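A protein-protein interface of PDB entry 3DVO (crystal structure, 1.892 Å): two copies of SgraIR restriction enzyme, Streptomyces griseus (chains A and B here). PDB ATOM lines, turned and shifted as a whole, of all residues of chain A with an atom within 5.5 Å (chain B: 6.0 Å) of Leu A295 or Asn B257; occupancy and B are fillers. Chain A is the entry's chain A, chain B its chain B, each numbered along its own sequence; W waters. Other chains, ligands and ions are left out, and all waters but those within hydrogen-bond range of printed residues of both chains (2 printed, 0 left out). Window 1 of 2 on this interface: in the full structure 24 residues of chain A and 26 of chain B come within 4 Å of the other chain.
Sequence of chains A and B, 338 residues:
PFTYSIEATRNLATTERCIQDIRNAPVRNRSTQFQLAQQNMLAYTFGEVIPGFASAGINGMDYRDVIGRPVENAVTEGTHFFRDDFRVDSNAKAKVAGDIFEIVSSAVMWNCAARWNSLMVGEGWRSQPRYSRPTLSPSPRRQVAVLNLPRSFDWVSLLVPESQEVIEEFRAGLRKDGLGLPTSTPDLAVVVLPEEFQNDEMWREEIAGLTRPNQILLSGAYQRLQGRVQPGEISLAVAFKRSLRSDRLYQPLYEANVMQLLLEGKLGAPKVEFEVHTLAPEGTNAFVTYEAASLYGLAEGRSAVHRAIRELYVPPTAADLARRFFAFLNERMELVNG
Water W2 lies within hydrogen-bond range of the backbone carbonyl oxygen of Ala B293 (2.6 Å), the side-chain hydroxyl of Tyr A254 (2.8 Å) and the side-chain amide nitrogen of Asn B257 (3.1 Å). Water W1 lies within hydrogen-bond range of the backbone carbonyl oxygen (O) of Ala A293 (2.7 Å), the side-chain hydroxyl (OH) of Tyr B254 (2.8 Å) and the side-chain amide nitrogen (ND2) of Asn A257 (3.1 Å).
Leu A295 touches just these residues of chain B: Leu B181, Asn B257, Leu B261 and Tyr B296. Asn B257 touches two residues of chain A. Of the printed residues of chain B, Tyr A254 touches Leu B253 and Asn B257. Printed residues of chain A within 4 Å of Leu B295: Asn A257 (3.97 Å). Of the printed residues of chain B, Ala A299 touches Tyr B296 and Ala B299. Printed residues of chain B within 4 Å of Tyr A296: Ala B299 (3.8 Å). Of the printed residues of chain B, Leu A298 touches Leu B261 (3.7 Å) and Tyr B296 (3.7 Å). Met B259 touches none of the printed residues of chain A. The nearest printed residue of chain A that does not touch Asn B257 is Asn A257 (7.5 Å).
Tyr A254 touches Asn B257, and with the chains exchanged Asn A257 touches Tyr B254. Asn A257 touches Leu B295, and with the chains exchanged Leu A295 touches Asn B257. Leu A295 touches Tyr B296, but with the chains exchanged Tyr A296 does not touch Leu B295 (5.6 Å). Ala A299 touches its own counterpart, Ala B299. 7 positions are printed for both chains. Of the 13 pairs that touch across the chains among the printed residues, 7 have their exchanged pair printed and touching as well.
Of the 10 printed residues of chain A, 6 touch a printed residue of chain B. Hydrophobic or aromatic side chains of chain A within 4 Å of the printed part of chain B: Tyr A254, Leu A295, Tyr A296, Leu A298 and Ala A299. Of the 18 printed residues of chain B, 8 touch a printed residue of chain A. Among the printed residues, 13 pairs touch across the chains. Among the printed residues, no Asp or Glu carboxylate lies within 4 Å of a Lys or Arg side-chain nitrogen of the other chain.
The backbone NH (N) of Leu A295 is in hydrogen-bond range of the side-chain amide oxygen (OD1) of Asn A257 (2.8 Å). The backbone carbonyl oxygen (O) of Leu B253 is in hydrogen-bond range of the side-chain amide nitrogen (ND2) of Asn B257 (2.9 Å). N of Leu B295 sits at hydrogen-bond distance from OD1 of Asn B257, at 2.8 Å.
Leu B253 touches Tyr A254. Tyr B254 touches Asn A257. Asn A257 touches Leu B295. Leu A295 touches Leu B181. CB of Asn B257 touches CD1 of Leu A295 (3.9 Å). Leu A295 touches Leu B261 (CD2 to CD1, 3.9 Å). Leu A295 touches Tyr B296. CD1 of Tyr A296 touches CB of Ala B299, 3.8 Å away. Leu B261 touches Leu A298. CA of Ala A299 touches CE1 of Tyr B296, 3.2 Å away.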
ATOM      1  N   TYR A 254      20.615  17.822   8.163  1.00  0.00           N
ATOM      2  CA  TYR A 254      19.531  17.528   9.078  1.00  0.00           C
ATOM      3  C   TYR A 254      19.858  17.971  10.522  1.00  0.00           C
ATOM      4  O   TYR A 254      19.054  18.646  11.167  1.00  0.00           O
ATOM      5  CB  TYR A 254      19.110  16.050   9.032  1.00  0.00           C
ATOM      6  CG  TYR A 254      17.912  15.864   9.919  1.00  0.00           C
ATOM      7  CD1 TYR A 254      16.648  16.299   9.517  1.00  0.00           C
ATOM      8  CD2 TYR A 254      18.062  15.374  11.202  1.00  0.00           C
ATOM      9  CE1 TYR A 254      15.557  16.176  10.353  1.00  0.00           C
ATOM     10  CE2 TYR A 254      16.985  15.252  12.048  1.00  0.00           C
ATOM     11  CZ  TYR A 254      15.739  15.660  11.629  1.00  0.00           C
ATOM     12  OH  TYR A 254      14.691  15.516  12.501  1.00  0.00           O
ATOM     13  N   ASN A 257      19.786  21.722  11.134  1.00  0.00           N
ATOM     14  CA  ASN A 257      18.426  22.253  11.271  1.00  0.00           C
ATOM     15  C   ASN A 257      17.855  22.039  12.680  1.00  0.00           C
ATOM     16  O   ASN A 257      17.162  22.891  13.225  1.00  0.00           O
ATOM     17  CB  ASN A 257      17.512  21.664  10.192  1.00  0.00           C
ATOM     18  CG  ASN A 257      17.599  22.423   8.908  1.00  0.00           C
ATOM     19  OD1 ASN A 257      17.106  23.549   8.801  1.00  0.00           O
ATOM     20  ND2 ASN A 257      18.235  21.828   7.922  1.00  0.00           N
ATOM     21  N   ALA A 293      18.200  27.124   3.058  1.00  0.00           N
ATOM     22  CA  ALA A 293      17.791  27.903   4.207  1.00  0.00           C
ATOM     23  C   ALA A 293      17.409  27.007   5.376  1.00  0.00           C
ATOM     24  O   ALA A 293      16.920  25.895   5.184  1.00  0.00           O
ATOM     25  CB  ALA A 293      16.610  28.778   3.832  1.00  0.00           C
ATOM     26  N   SER A 294      17.614  27.510   6.593  1.00  0.00           N
ATOM     27  CA  SER A 294      17.188  26.816   7.798  1.00  0.00           C
ATOM     28  C   SER A 294      15.667  26.632   7.792  1.00  0.00           C
ATOM     29  O   SER A 294      14.923  27.593   7.635  1.00  0.00           O
ATOM     30  CB  SER A 294      17.628  27.621   9.018  1.00  0.00           C
ATOM     31  OG  SER A 294      17.217  27.017  10.230  1.00  0.00           O
ATOM     32  N   LEU A 295      15.195  25.403   7.973  1.00  0.00           N
ATOM     33  CA  LEU A 295      13.752  25.169   7.942  1.00  0.00           C
ATOM     34  C   LEU A 295      13.011  25.917   9.063  1.00  0.00           C
ATOM     35  O   LEU A 295      11.922  26.474   8.861  1.00  0.00           O
ATOM     36  CB  LEU A 295      13.445  23.686   8.018  1.00  0.00           C
ATOM     37  CG  LEU A 295      14.139  22.834   6.960  1.00  0.00           C
ATOM     38  CD1 LEU A 295      13.573  21.420   7.018  1.00  0.00           C
ATOM     39  CD2 LEU A 295      13.958  23.437   5.577  1.00  0.00           C
ATOM     40  N   TYR A 296      13.606  25.926  10.247  1.00  0.00           N
ATOM     41  CA  TYR A 296      13.034  26.658  11.363  1.00  0.00           C
ATOM     42  C   TYR A 296      12.989  28.141  11.020  1.00  0.00           C
ATOM     43  O   TYR A 296      12.023  28.834  11.333  1.00  0.00           O
ATOM     44  CB  TYR A 296      13.845  26.406  12.645  1.00  0.00           C
ATOM     45  CG  TYR A 296      13.886  27.580  13.592  1.00  0.00           C
ATOM     46  CD1 TYR A 296      12.846  27.816  14.486  1.00  0.00           C
ATOM     47  CD2 TYR A 296      14.962  28.456  13.587  1.00  0.00           C
ATOM     48  CE1 TYR A 296      12.874  28.902  15.346  1.00  0.00           C
ATOM     49  CE2 TYR A 296      15.000  29.544  14.447  1.00  0.00           C
ATOM     50  CZ  TYR A 296      13.953  29.761  15.317  1.00  0.00           C
ATOM     51  OH  TYR A 296      13.996  30.838  16.169  1.00  0.00           O
ATOM     52  N   GLY A 297      14.051  28.626  10.383  1.00  0.00           N
ATOM     53  CA  GLY A 297      14.102  30.004   9.933  1.00  0.00           C
ATOM     54  C   GLY A 297      12.890  30.331   9.089  1.00  0.00           C
ATOM     55  O   GLY A 297      12.229  31.347   9.305  1.00  0.00           O
ATOM     56  N   LEU A 298      12.589  29.460   8.130  1.00  0.00           N
ATOM     57  CA  LEU A 298      11.410  29.641   7.293  1.00  0.00           C
ATOM     58  C   LEU A 298      10.140  29.532   8.111  1.00  0.00           C
ATOM     59  O   LEU A 298       9.231  30.347   7.971  1.00  0.00           O
ATOM     60  CB  LEU A 298      11.384  28.608   6.174  1.00  0.00           C
ATOM     61  CG  LEU A 298      12.642  28.622   5.322  1.00  0.00           C
ATOM     62  CD1 LEU A 298      12.599  27.493   4.325  1.00  0.00           C
ATOM     63  CD2 LEU A 298      12.771  29.975   4.627  1.00  0.00           C
ATOM     64  N   ALA A 299      10.070  28.517   8.959  1.00  0.00           N
ATOM     65  CA  ALA A 299       8.860  28.280   9.736  1.00  0.00           C
ATOM     66  C   ALA A 299       8.511  29.505  10.574  1.00  0.00           C
ATOM     67  O   ALA A 299       7.372  29.664  11.015  1.00  0.00           O
ATOM     68  CB  ALA A 299       9.013  27.044  10.602  1.00  0.00           C
ATOM     69  N   GLU A 300       9.499  30.377  10.767  1.00  0.00           N
ATOM     70  CA  GLU A 300       9.301  31.644  11.468  1.00  0.00           C
ATOM     71  C   GLU A 300       8.149  32.448  10.876  1.00  0.00           C
ATOM     72  O   GLU A 300       8.336  33.595  10.459  1.00  0.00           O
ATOM     73  CB  GLU A 300      10.578  32.485  11.411  1.00  0.00           C
ATOM     74  CG  GLU A 300      10.621  33.610  12.430  1.00  0.00           C
ATOM     75  CD  GLU A 300      10.612  33.083  13.852  1.00  0.00           C
ATOM     76  OE1 GLU A 300      11.055  31.932  14.056  1.00  0.00           O
ATOM     77  OE2 GLU A 300      10.161  33.814  14.762  1.00  0.00           O
ATOM     78  N   LEU B 181      16.089  26.478  -1.552  1.00  0.00           N
ATOM     79  CA  LEU B 181      15.437  25.351  -0.916  1.00  0.00           C
ATOM     80  C   LEU B 181      15.305  24.245  -1.934  1.00  0.00           C
ATOM     81  O   LEU B 181      14.207  23.941  -2.389  1.00  0.00           O
ATOM     82  CB  LEU B 181      14.073  25.745  -0.333  1.00  0.00           C
ATOM     83  CG  LEU B 181      13.436  24.690   0.583  1.00  0.00           C
ATOM     84  CD1 LEU B 181      14.305  24.399   1.786  1.00  0.00           C
ATOM     85  CD2 LEU B 181      12.035  25.099   1.029  1.00  0.00           C
ATOM     86  N   PRO B 252      16.202  10.569   3.530  1.00  0.00           N
ATOM     87  CA  PRO B 252      14.746  10.438   3.517  1.00  0.00           C
ATOM     88  C   PRO B 252      14.099  11.402   4.514  1.00  0.00           C
ATOM     89  O   PRO B 252      13.082  12.038   4.225  1.00  0.00           O
ATOM     90  CB  PRO B 252      14.524   8.989   3.949  1.00  0.00           C
ATOM     91  CG  PRO B 252      15.770   8.268   3.485  1.00  0.00           C
ATOM     92  CD  PRO B 252      16.879   9.269   3.714  1.00  0.00           C
ATOM     93  N   LEU B 253      14.710  11.523   5.683  1.00  0.00           N
ATOM     94  CA  LEU B 253      14.140  12.344   6.745  1.00  0.00           C
ATOM     95  C   LEU B 253      14.190  13.815   6.337  1.00  0.00           C
ATOM     96  O   LEU B 253      13.251  14.575   6.596  1.00  0.00           O
ATOM     97  CB  LEU B 253      14.897  12.090   8.056  1.00  0.00           C
ATOM     98  CG  LEU B 253      14.444  12.718   9.381  1.00  0.00           C
ATOM     99  CD1 LEU B 253      12.965  12.521   9.613  1.00  0.00           C
ATOM    100  CD2 LEU B 253      15.233  12.115  10.524  1.00  0.00           C
ATOM    101  N   TYR B 254      15.284  14.223   5.696  1.00  0.00           N
ATOM    102  CA  TYR B 254      15.403  15.611   5.270  1.00  0.00           C
ATOM    103  C   TYR B 254      14.429  15.906   4.131  1.00  0.00           C
ATOM    104  O   TYR B 254      13.681  16.888   4.181  1.00  0.00           O
ATOM    105  CB  TYR B 254      16.834  15.999   4.870  1.00  0.00           C
ATOM    106  CG  TYR B 254      16.892  17.457   4.463  1.00  0.00           C
ATOM    107  CD1 TYR B 254      16.925  18.461   5.423  1.00  0.00           C
ATOM    108  CD2 TYR B 254      16.829  17.834   3.128  1.00  0.00           C
ATOM    109  CE1 TYR B 254      16.950  19.785   5.071  1.00  0.00           C
ATOM    110  CE2 TYR B 254      16.852  19.159   2.764  1.00  0.00           C
ATOM    111  CZ  TYR B 254      16.911  20.135   3.740  1.00  0.00           C
ATOM    112  OH  TYR B 254      16.925  21.473   3.390  1.00  0.00           O
ATOM    113  N   GLU B 255      14.426  15.056   3.111  1.00  0.00           N
ATOM    114  CA  GLU B 255      13.492  15.237   2.002  1.00  0.00           C
ATOM    115  C   GLU B 255      12.035  15.208   2.459  1.00  0.00           C
ATOM    116  O   GLU B 255      11.221  15.970   1.956  1.00  0.00           O
ATOM    117  CB  GLU B 255      13.702  14.208   0.892  1.00  0.00           C
ATOM    118  CG  GLU B 255      13.052  14.643  -0.420  1.00  0.00           C
ATOM    119  CD  GLU B 255      13.642  15.951  -0.972  1.00  0.00           C
ATOM    120  OE1 GLU B 255      14.879  16.157  -0.856  1.00  0.00           O
ATOM    121  OE2 GLU B 255      12.870  16.769  -1.525  1.00  0.00           O
ATOM    122  N   ALA B 256      11.700  14.347   3.416  1.00  0.00           N
ATOM    123  CA  ALA B 256      10.322  14.305   3.893  1.00  0.00           C
ATOM    124  C   ALA B 256       9.950  15.653   4.457  1.00  0.00           C
ATOM    125  O   ALA B 256       8.847  16.156   4.247  1.00  0.00           O
ATOM    126  CB  ALA B 256      10.137  13.223   4.941  1.00  0.00           C
ATOM    127  N   ASN B 257      10.900  16.247   5.161  1.00  0.00           N
ATOM    128  CA  ASN B 257      10.707  17.546   5.767  1.00  0.00           C
ATOM    129  C   ASN B 257      10.489  18.668   4.756  1.00  0.00           C
ATOM    130  O   ASN B 257       9.585  19.478   4.905  1.00  0.00           O
ATOM    131  CB  ASN B 257      11.903  17.869   6.657  1.00  0.00           C
ATOM    132  CG  ASN B 257      11.642  17.533   8.079  1.00  0.00           C
ATOM    133  OD1 ASN B 257      10.901  18.239   8.760  1.00  0.00           O
ATOM    134  ND2 ASN B 257      12.210  16.429   8.539  1.00  0.00           N
ATOM    135  N   VAL B 258      11.315  18.708   3.725  1.00  0.00           N
ATOM    136  CA  VAL B 258      11.136  19.714   2.679  1.00  0.00           C
ATOM    137  C   VAL B 258       9.824  19.507   1.915  1.00  0.00           C
ATOM    138  O   VAL B 258       9.113  20.468   1.623  1.00  0.00           O
ATOM    139  CB  VAL B 258      12.346  19.768   1.752  1.00  0.00           C
ATOM    140  CG1 VAL B 258      12.118  20.754   0.610  1.00  0.00           C
ATOM    141  CG2 VAL B 258      13.586  20.177   2.562  1.00  0.00           C
ATOM    142  N   MET B 259       9.480  18.258   1.625  1.00  0.00           N
ATOM    143  CA  MET B 259       8.199  17.976   0.976  1.00  0.00           C
ATOM    144  C   MET B 259       7.028  18.497   1.782  1.00  0.00           C
ATOM    145  O   MET B 259       6.071  19.018   1.223  1.00  0.00           O
ATOM    146  CB  MET B 259       8.020  16.480   0.735  1.00  0.00           C
ATOM    147  CG  MET B 259       8.783  15.965  -0.471  1.00  0.00           C
ATOM    148  SD  MET B 259       8.479  14.204  -0.655  1.00  0.00           S
ATOM    149  CE  MET B 259       6.697  14.192  -0.768  1.00  0.00           C
ATOM    150  N   GLN B 260       7.090  18.353   3.097  1.00  0.00           N
ATOM    151  CA  GLN B 260       5.971  18.772   3.925  1.00  0.00           C
ATOM    152  C   GLN B 260       5.887  20.296   4.045  1.00  0.00           C
ATOM    153  O   GLN B 260       4.782  20.871   4.068  1.00  0.00           O
ATOM    154  CB  GLN B 260       6.031  18.081   5.292  1.00  0.00           C
ATOM    155  CG  GLN B 260       5.570  16.627   5.248  1.00  0.00           C
ATOM    156  CD  GLN B 260       6.261  15.745   6.274  1.00  0.00           C
ATOM    157  OE1 GLN B 260       6.849  16.231   7.244  1.00  0.00           O
ATOM    158  NE2 GLN B 260       6.203  14.429   6.053  1.00  0.00           N
ATOM    159  N   LEU B 261       7.052  20.940   4.106  1.00  0.00           N
ATOM    160  CA  LEU B 261       7.135  22.398   4.101  1.00  0.00           C
ATOM    161  C   LEU B 261       6.443  22.924   2.853  1.00  0.00           C
ATOM    162  O   LEU B 261       5.589  23.805   2.916  1.00  0.00           O
ATOM    163  CB  LEU B 261       8.599  22.856   4.113  1.00  0.00           C
ATOM    164  CG  LEU B 261       8.923  24.356   4.223  1.00  0.00           C
ATOM    165  CD1 LEU B 261      10.346  24.575   4.791  1.00  0.00           C
ATOM    166  CD2 LEU B 261       8.760  25.103   2.890  1.00  0.00           C
ATOM    167  N   LEU B 262       6.807  22.358   1.711  1.00  0.00           N
ATOM    168  CA  LEU B 262       6.313  22.881   0.454  1.00  0.00           C
ATOM    169  C   LEU B 262       4.856  22.494   0.227  1.00  0.00           C
ATOM    170  O   LEU B 262       4.029  23.354  -0.046  1.00  0.00           O
ATOM    171  CB  LEU B 262       7.204  22.428  -0.706  1.00  0.00           C
ATOM    172  CG  LEU B 262       8.632  22.982  -0.722  1.00  0.00           C
ATOM    173  CD1 LEU B 262       9.434  22.335  -1.830  1.00  0.00           C
ATOM    174  CD2 LEU B 262       8.648  24.499  -0.883  1.00  0.00           C
ATOM    175  N   ALA B 293       9.406  14.459  14.668  1.00  0.00           N
ATOM    176  CA  ALA B 293       8.373  15.315  14.115  1.00  0.00           C
ATOM    177  C   ALA B 293       8.883  16.208  12.986  1.00  0.00           C
ATOM    178  O   ALA B 293      10.047  16.622  12.955  1.00  0.00           O
ATOM    179  CB  ALA B 293       7.726  16.164  15.223  1.00  0.00           C
ATOM    180  N   SER B 294       7.977  16.503  12.065  1.00  0.00           N
ATOM    181  CA  SER B 294       8.214  17.438  10.980  1.00  0.00           C
ATOM    182  C   SER B 294       8.618  18.781  11.572  1.00  0.00           C
ATOM    183  O   SER B 294       7.915  19.315  12.428  1.00  0.00           O
ATOM    184  CB  SER B 294       6.914  17.598  10.187  1.00  0.00           C
ATOM    185  OG  SER B 294       7.130  18.293   8.982  1.00  0.00           O
ATOM    186  N   LEU B 295       9.738  19.326  11.103  1.00  0.00           N
ATOM    187  CA  LEU B 295      10.318  20.559  11.657  1.00  0.00           C
ATOM    188  C   LEU B 295       9.522  21.817  11.350  1.00  0.00           C
ATOM    189  O   LEU B 295       9.261  22.627  12.238  1.00  0.00           O
ATOM    190  CB  LEU B 295      11.744  20.747  11.150  1.00  0.00           C
ATOM    191  CG  LEU B 295      12.661  19.590  11.537  1.00  0.00           C
ATOM    192  CD1 LEU B 295      14.084  19.998  11.320  1.00  0.00           C
ATOM    193  CD2 LEU B 295      12.422  19.213  12.990  1.00  0.00           C
ATOM    194  N   TYR B 296       9.163  21.990  10.086  1.00  0.00           N
ATOM    195  CA  TYR B 296       8.468  23.188   9.662  1.00  0.00           C
ATOM    196  C   TYR B 296       7.181  23.299  10.438  1.00  0.00           C
ATOM    197  O   TYR B 296       6.896  24.332  11.047  1.00  0.00           O
ATOM    198  CB  TYR B 296       8.160  23.156   8.169  1.00  0.00           C
ATOM    199  CG  TYR B 296       7.602  24.472   7.669  1.00  0.00           C
ATOM    200  CD1 TYR B 296       8.429  25.579   7.504  1.00  0.00           C
ATOM    201  CD2 TYR B 296       6.247  24.616   7.386  1.00  0.00           C
ATOM    202  CE1 TYR B 296       7.925  26.790   7.054  1.00  0.00           C
ATOM    203  CE2 TYR B 296       5.735  25.820   6.934  1.00  0.00           C
ATOM    204  CZ  TYR B 296       6.577  26.902   6.770  1.00  0.00           C
ATOM    205  OH  TYR B 296       6.065  28.103   6.325  1.00  0.00           O
ATOM    206  N   ALA B 299       7.993  24.284  14.181  1.00  0.00           N
ATOM    207  CA  ALA B 299       8.437  25.659  14.359  1.00  0.00           C
ATOM    208  C   ALA B 299       7.383  26.711  14.004  1.00  0.00           C
ATOM    209  O   ALA B 299       7.427  27.822  14.523  1.00  0.00           O
ATOM    210  CB  ALA B 299       9.711  25.892  13.565  1.00  0.00           C
ATOM    211  N   ALA B 308       7.632  13.306  10.406  1.00  0.00           N
ATOM    212  CA  ALA B 308       8.209  13.519   9.092  1.00  0.00           C
ATOM    213  C   ALA B 308       8.022  12.243   8.298  1.00  0.00           C
ATOM    214  O   ALA B 308       7.522  12.268   7.174  1.00  0.00           O
ATOM    215  CB  ALA B 308       9.702  13.847   9.209  1.00  0.00           C
HETATM  216  O   HOH W   1      17.702  23.339   5.268  1.00  0.00           O
HETATM  217  O   HOH W   2      12.074  15.700  11.528  1.00  0.00           O
